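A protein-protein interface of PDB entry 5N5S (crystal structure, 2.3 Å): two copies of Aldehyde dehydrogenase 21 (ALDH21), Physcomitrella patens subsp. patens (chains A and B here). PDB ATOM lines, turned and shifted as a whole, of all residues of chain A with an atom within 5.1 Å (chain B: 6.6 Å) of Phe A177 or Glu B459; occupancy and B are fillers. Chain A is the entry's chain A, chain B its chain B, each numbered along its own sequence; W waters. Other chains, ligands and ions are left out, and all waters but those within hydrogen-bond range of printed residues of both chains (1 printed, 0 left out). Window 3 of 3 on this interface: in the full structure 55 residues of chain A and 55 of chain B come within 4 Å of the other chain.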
ATOM      1  N   LYS A 175      10.964   5.378  -5.062  1.00  0.00           N
ATOM      2  CA  LYS A 175      11.304   6.637  -5.727  1.00  0.00           C
ATOM      3  C   LYS A 175      10.324   7.712  -5.287  1.00  0.00           C
ATOM      4  O   LYS A 175       9.233   7.396  -4.806  1.00  0.00           O
ATOM      5  CB  LYS A 175      11.249   6.470  -7.248  1.00  0.00           C
ATOM      6  CG  LYS A 175      12.534   6.812  -7.954  1.00  0.00           C
ATOM      7  CD  LYS A 175      12.521   6.324  -9.406  1.00  0.00           C
ATOM      8  CE  LYS A 175      12.161   7.403 -10.396  1.00  0.00           C
ATOM      9  NZ  LYS A 175      12.346   6.938 -11.791  1.00  0.00           N
ATOM     10  N   LYS A 176      10.722   8.975  -5.431  1.00  0.00           N
ATOM     11  CA  LYS A 176       9.891  10.106  -5.035  1.00  0.00           C
ATOM     12  C   LYS A 176       9.542  10.903  -6.266  1.00  0.00           C
ATOM     13  O   LYS A 176      10.419  11.172  -7.101  1.00  0.00           O
ATOM     14  CB  LYS A 176      10.573  10.974  -3.951  1.00  0.00           C
ATOM     15  CG  LYS A 176      10.843  10.224  -2.655  1.00  0.00           C
ATOM     16  CD  LYS A 176      10.994  11.162  -1.482  1.00  0.00           C
ATOM     17  CE  LYS A 176      11.757  10.541  -0.331  1.00  0.00           C
ATOM     18  NZ  LYS A 176      13.230  10.492  -0.592  1.00  0.00           N
ATOM     19  N   PHE A 177       8.250  11.252  -6.391  1.00  0.00           N
ATOM     20  CA  PHE A 177       7.703  11.960  -7.542  1.00  0.00           C
ATOM     21  C   PHE A 177       7.052  13.276  -7.125  1.00  0.00           C
ATOM     22  O   PHE A 177       6.453  13.322  -6.040  1.00  0.00           O
ATOM     23  CB  PHE A 177       6.658  11.053  -8.251  1.00  0.00           C
ATOM     24  CG  PHE A 177       7.243   9.822  -8.924  1.00  0.00           C
ATOM     25  CD1 PHE A 177       7.536   8.674  -8.189  1.00  0.00           C
ATOM     26  CD2 PHE A 177       7.500   9.811 -10.285  1.00  0.00           C
ATOM     27  CE1 PHE A 177       8.124   7.563  -8.802  1.00  0.00           C
ATOM     28  CE2 PHE A 177       8.056   8.685 -10.900  1.00  0.00           C
ATOM     29  CZ  PHE A 177       8.362   7.569 -10.156  1.00  0.00           C
ATOM     30  N   PRO A 178       7.082  14.343  -7.982  1.00  0.00           N
ATOM     31  CA  PRO A 178       6.376  15.598  -7.612  1.00  0.00           C
ATOM     32  C   PRO A 178       4.912  15.357  -7.197  1.00  0.00           C
ATOM     33  O   PRO A 178       4.233  14.514  -7.793  1.00  0.00           O
ATOM     34  CB  PRO A 178       6.433  16.432  -8.902  1.00  0.00           C
ATOM     35  CG  PRO A 178       7.616  15.886  -9.660  1.00  0.00           C
ATOM     36  CD  PRO A 178       7.720  14.439  -9.318  1.00  0.00           C
ATOM     37  N   ILE A 179       4.439  16.071  -6.171  1.00  0.00           N
ATOM     38  CA  ILE A 179       3.066  15.963  -5.658  1.00  0.00           C
ATOM     39  C   ILE A 179       2.038  16.513  -6.676  1.00  0.00           C
ATOM     40  O   ILE A 179       0.946  15.951  -6.813  1.00  0.00           O
ATOM     41  CB  ILE A 179       2.932  16.600  -4.235  1.00  0.00           C
ATOM     42  CG1 ILE A 179       1.660  16.096  -3.505  1.00  0.00           C
ATOM     43  CG2 ILE A 179       3.028  18.156  -4.246  1.00  0.00           C
ATOM     44  CD1 ILE A 179       1.564  16.460  -1.992  1.00  0.00           C
ATOM     45  N   MET A 501       6.639  18.103  -0.892  1.00  0.00           N
ATOM     46  CA  MET A 501       6.329  18.311  -2.309  1.00  0.00           C
ATOM     47  C   MET A 501       6.615  17.063  -3.153  1.00  0.00           C
ATOM     48  O   MET A 501       6.504  17.098  -4.372  1.00  0.00           O
ATOM     49  CB  MET A 501       7.081  19.536  -2.849  1.00  0.00           C
ATOM     50  CG  MET A 501       6.682  20.804  -2.157  1.00  0.00           C
ATOM     51  SD  MET A 501       7.543  22.232  -2.791  1.00  0.00           S
ATOM     52  CE  MET A 501       6.894  23.518  -1.668  1.00  0.00           C
ATOM     53  N   LEU A 502       6.976  15.966  -2.496  1.00  0.00           N
ATOM     54  CA  LEU A 502       7.272  14.692  -3.131  1.00  0.00           C
ATOM     55  C   LEU A 502       6.377  13.602  -2.558  1.00  0.00           C
ATOM     56  O   LEU A 502       6.140  13.559  -1.351  1.00  0.00           O
ATOM     57  CB  LEU A 502       8.754  14.306  -2.940  1.00  0.00           C
ATOM     58  CG  LEU A 502       9.782  15.082  -3.763  1.00  0.00           C
ATOM     59  CD1 LEU A 502      11.150  14.983  -3.140  1.00  0.00           C
ATOM     60  CD2 LEU A 502       9.826  14.613  -5.221  1.00  0.00           C
ATOM     61  N   GLU A 503       5.890  12.719  -3.435  1.00  0.00           N
ATOM     62  CA  GLU A 503       5.075  11.558  -3.093  1.00  0.00           C
ATOM     63  C   GLU A 503       5.928  10.316  -3.312  1.00  0.00           C
ATOM     64  O   GLU A 503       6.676  10.239  -4.286  1.00  0.00           O
ATOM     65  CB  GLU A 503       3.800  11.486  -3.960  1.00  0.00           C
ATOM     66  CG  GLU A 503       2.711  12.473  -3.561  1.00  0.00           C
ATOM     67  CD  GLU A 503       1.689  12.030  -2.526  1.00  0.00           C
ATOM     68  OE1 GLU A 503       0.519  12.464  -2.644  1.00  0.00           O
ATOM     69  OE2 GLU A 503       2.038  11.243  -1.615  1.00  0.00           O
ATOM     70  N   THR A 504       5.811   9.351  -2.406  1.00  0.00           N
ATOM     71  CA  THR A 504       6.535   8.085  -2.437  1.00  0.00           C
ATOM     72  C   THR A 504       5.841   7.061  -3.352  1.00  0.00           C
ATOM     73  O   THR A 504       4.638   6.841  -3.225  1.00  0.00           O
ATOM     74  CB  THR A 504       6.678   7.566  -0.993  1.00  0.00           C
ATOM     75  OG1 THR A 504       7.547   8.448  -0.288  1.00  0.00           O
ATOM     76  CG2 THR A 504       7.226   6.154  -0.919  1.00  0.00           C
ATOM     77  N   LYS A 505       6.610   6.414  -4.239  1.00  0.00           N
ATOM     78  CA  LYS A 505       6.107   5.329  -5.085  1.00  0.00           C
ATOM     79  C   LYS A 505       7.063   4.150  -5.002  1.00  0.00           C
ATOM     80  O   LYS A 505       8.271   4.330  -5.105  1.00  0.00           O
ATOM     81  CB  LYS A 505       5.924   5.764  -6.541  1.00  0.00           C
ATOM     82  CG  LYS A 505       4.948   4.844  -7.290  1.00  0.00           C
ATOM     83  CD  LYS A 505       4.872   5.105  -8.778  1.00  0.00           C
ATOM     84  CE  LYS A 505       4.351   6.484  -9.111  1.00  0.00           C
ATOM     85  NZ  LYS A 505       4.388   6.740 -10.568  1.00  0.00           N
ATOM     86  N   ALA B 454       8.088  -1.937 -18.103  1.00  0.00           N
ATOM     87  CA  ALA B 454       8.151  -2.064 -16.643  1.00  0.00           C
ATOM     88  C   ALA B 454       8.456  -0.713 -15.992  1.00  0.00           C
ATOM     89  O   ALA B 454       7.772  -0.326 -15.047  1.00  0.00           O
ATOM     90  CB  ALA B 454       9.219  -3.075 -16.256  1.00  0.00           C
ATOM     91  N   PHE B 455       9.451   0.021 -16.531  1.00  0.00           N
ATOM     92  CA  PHE B 455       9.860   1.309 -15.991  1.00  0.00           C
ATOM     93  C   PHE B 455       8.975   2.465 -16.471  1.00  0.00           C
ATOM     94  O   PHE B 455       8.873   3.452 -15.753  1.00  0.00           O
ATOM     95  CB  PHE B 455      11.361   1.554 -16.227  1.00  0.00           C
ATOM     96  CG  PHE B 455      12.157   0.779 -15.193  1.00  0.00           C
ATOM     97  CD1 PHE B 455      12.424  -0.578 -15.366  1.00  0.00           C
ATOM     98  CD2 PHE B 455      12.556   1.382 -14.002  1.00  0.00           C
ATOM     99  CE1 PHE B 455      13.090  -1.313 -14.381  1.00  0.00           C
ATOM    100  CE2 PHE B 455      13.223   0.646 -13.014  1.00  0.00           C
ATOM    101  CZ  PHE B 455      13.485  -0.694 -13.209  1.00  0.00           C
ATOM    102  N   TYR B 456       8.301   2.334 -17.636  1.00  0.00           N
ATOM    103  CA  TYR B 456       7.335   3.329 -18.118  1.00  0.00           C
ATOM    104  C   TYR B 456       6.140   3.315 -17.148  1.00  0.00           C
ATOM    105  O   TYR B 456       5.671   4.379 -16.738  1.00  0.00           O
ATOM    106  CB  TYR B 456       6.854   3.022 -19.565  1.00  0.00           C
ATOM    107  CG  TYR B 456       5.851   4.036 -20.083  1.00  0.00           C
ATOM    108  CD1 TYR B 456       4.481   3.864 -19.872  1.00  0.00           C
ATOM    109  CD2 TYR B 456       6.271   5.194 -20.733  1.00  0.00           C
ATOM    110  CE1 TYR B 456       3.557   4.819 -20.292  1.00  0.00           C
ATOM    111  CE2 TYR B 456       5.352   6.144 -21.180  1.00  0.00           C
ATOM    112  CZ  TYR B 456       3.997   5.952 -20.953  1.00  0.00           C
ATOM    113  OH  TYR B 456       3.088   6.891 -21.369  1.00  0.00           O
ATOM    114  N   ALA B 457       5.671   2.106 -16.764  1.00  0.00           N
ATOM    115  CA  ALA B 457       4.556   1.901 -15.843  1.00  0.00           C
ATOM    116  C   ALA B 457       4.894   2.452 -14.463  1.00  0.00           C
ATOM    117  O   ALA B 457       4.066   3.154 -13.877  1.00  0.00           O
ATOM    118  CB  ALA B 457       4.203   0.424 -15.757  1.00  0.00           C
ATOM    119  N   PHE B 458       6.126   2.198 -13.971  1.00  0.00           N
ATOM    120  CA  PHE B 458       6.570   2.702 -12.678  1.00  0.00           C
ATOM    121  C   PHE B 458       6.542   4.234 -12.669  1.00  0.00           C
ATOM    122  O   PHE B 458       6.056   4.825 -11.725  1.00  0.00           O
ATOM    123  CB  PHE B 458       7.962   2.145 -12.314  1.00  0.00           C
ATOM    124  CG  PHE B 458       8.578   2.637 -11.009  1.00  0.00           C
ATOM    125  CD1 PHE B 458       7.803   2.775  -9.858  1.00  0.00           C
ATOM    126  CD2 PHE B 458       9.949   2.868 -10.911  1.00  0.00           C
ATOM    127  CE1 PHE B 458       8.371   3.207  -8.658  1.00  0.00           C
ATOM    128  CE2 PHE B 458      10.518   3.291  -9.708  1.00  0.00           C
ATOM    129  CZ  PHE B 458       9.726   3.454  -8.587  1.00  0.00           C
ATOM    130  N   GLU B 459       6.976   4.852 -13.753  1.00  0.00           N
ATOM    131  CA  GLU B 459       7.018   6.294 -13.911  1.00  0.00           C
ATOM    132  C   GLU B 459       5.644   6.949 -14.042  1.00  0.00           C
ATOM    133  O   GLU B 459       5.419   8.002 -13.422  1.00  0.00           O
ATOM    134  CB  GLU B 459       7.877   6.632 -15.152  1.00  0.00           C
ATOM    135  CG  GLU B 459       8.404   8.063 -15.213  1.00  0.00           C
ATOM    136  CD  GLU B 459       9.448   8.469 -14.180  1.00  0.00           C
ATOM    137  OE1 GLU B 459       9.602   9.692 -13.954  1.00  0.00           O
ATOM    138  OE2 GLU B 459      10.101   7.574 -13.591  1.00  0.00           O
ATOM    139  N   HIS B 460       4.730   6.338 -14.837  1.00  0.00           N
ATOM    140  CA  HIS B 460       3.459   6.957 -15.192  1.00  0.00           C
ATOM    141  C   HIS B 460       2.194   6.425 -14.496  1.00  0.00           C
ATOM    142  O   HIS B 460       1.157   7.094 -14.605  1.00  0.00           O
ATOM    143  CB  HIS B 460       3.298   6.933 -16.720  1.00  0.00           C
ATOM    144  CG  HIS B 460       4.374   7.737 -17.382  1.00  0.00           C
ATOM    145  ND1 HIS B 460       5.423   7.127 -18.041  1.00  0.00           N
ATOM    146  CD2 HIS B 460       4.611   9.071 -17.327  1.00  0.00           C
ATOM    147  CE1 HIS B 460       6.207   8.111 -18.455  1.00  0.00           C
ATOM    148  NE2 HIS B 460       5.760   9.297 -18.042  1.00  0.00           N
ATOM    149  N   MET B 461       2.265   5.314 -13.740  1.00  0.00           N
ATOM    150  CA  MET B 461       1.088   4.845 -13.001  1.00  0.00           C
ATOM    151  C   MET B 461       0.871   5.710 -11.756  1.00  0.00           C
ATOM    152  O   MET B 461       1.762   5.820 -10.910  1.00  0.00           O
ATOM    153  CB  MET B 461       1.170   3.352 -12.675  1.00  0.00           C
ATOM    154  CG  MET B 461       0.778   2.489 -13.856  1.00  0.00           C
ATOM    155  SD  MET B 461       1.089   0.744 -13.560  1.00  0.00           S
ATOM    156  CE  MET B 461      -0.097   0.026 -14.703  1.00  0.00           C
ATOM    157  N   GLU B 462      -0.296   6.375 -11.686  1.00  0.00           N
ATOM    158  CA  GLU B 462      -0.677   7.309 -10.620  1.00  0.00           C
ATOM    159  C   GLU B 462      -1.158   6.584  -9.365  1.00  0.00           C
ATOM    160  O   GLU B 462      -2.317   6.697  -8.965  1.00  0.00           O
ATOM    161  CB  GLU B 462      -1.709   8.326 -11.153  1.00  0.00           C
ATOM    162  CG  GLU B 462      -1.174   9.169 -12.303  1.00  0.00           C
ATOM    163  CD  GLU B 462      -2.166  10.010 -13.086  1.00  0.00           C
ATOM    164  OE1 GLU B 462      -3.374   9.678 -13.100  1.00  0.00           O
ATOM    165  OE2 GLU B 462      -1.715  10.980 -13.734  1.00  0.00           O
ATOM    166  N   VAL B 466       3.396   0.050  -7.527  1.00  0.00           N
ATOM    167  CA  VAL B 466       3.309  -0.623  -8.830  1.00  0.00           C
ATOM    168  C   VAL B 466       3.845  -2.041  -8.608  1.00  0.00           C
ATOM    169  O   VAL B 466       5.007  -2.208  -8.213  1.00  0.00           O
ATOM    170  CB  VAL B 466       4.076   0.130  -9.967  1.00  0.00           C
ATOM    171  CG1 VAL B 466       4.001  -0.628 -11.291  1.00  0.00           C
ATOM    172  CG2 VAL B 466       3.551   1.546 -10.145  1.00  0.00           C
HETATM  173  O   HOH W   1      10.966   4.747 -14.000  1.00  0.00           O
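Of the 10 printed residues of chain A, 3 touch a printed residue of chain B.
Hydrophobic or aromatic side chains of chain A within 4 Å of the printed part of chain B: Phe A177.
Along chain A the printed residues that touch a printed residue of chain B span positions 175 to 505.
Hydrophobic or aromatic side chains of chain B that line the printed part of chain A: Phe B458.
NZ of Lys A175 lies within salt-bridge range of OE2 of Glu B459 (2.9 Å).
The side-chain amino group (NZ) of Lys A505 sits at hydrogen-bond distance from the backbone carbonyl oxygen (O) of Phe B458 (2.8 Å).
O of Glu B459 sits at hydrogen-bond distance from NZ of Lys A505 (3.3 Å).
The side-chain amino group of Lys A505 lies within hydrogen-bond range of the backbone carbonyl oxygen of Met B461 (2.8 Å).
Of chain B, only Phe B458 and Glu B459 come within 4 Å of Phe A177.
Glu B459 touches just these residues of chain A: Lys A175, Phe A177 and Lys A505.
Printed residues of chain B within 4 Å of Lys A505: Phe B458, Glu B459 and Met B461.
Of the printed residues of chain A, Met B461 touches Lys A505 (2.8 Å).
Printed residues of chain B within 4 Å of Lys A175: Phe B458 (3.6 Å) and Glu B459 (2.9 Å).
Of the printed residues of chain A, Phe B458 touches Lys A175 (3.6 Å), Phe A177 (3.9 Å) and Lys A505 (2.8 Å).
N of Lys A505 sits at hydrogen-bond distance from O of Lys A175 (2.9 Å).
The backbone carbonyl oxygen (O) of Phe A177 is in hydrogen-bond range of the backbone NH (N) of Glu A503 (2.7 Å).
Water W1 lies within hydrogen-bond range of OE2 of Glu B459 (3.0 Å), O of Phe B455 (3.0 Å) and NZ of Lys A175 (3.4 Å).
CB of Lys A175 touches CZ of Phe B458, 3.6 Å away.
Phe B458 touches Phe A177 (O to CZ, 3.9 Å).
Glu B459 touches Phe A177 (OE2 to CE2, 3.6 Å).
No position is printed for both chains.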
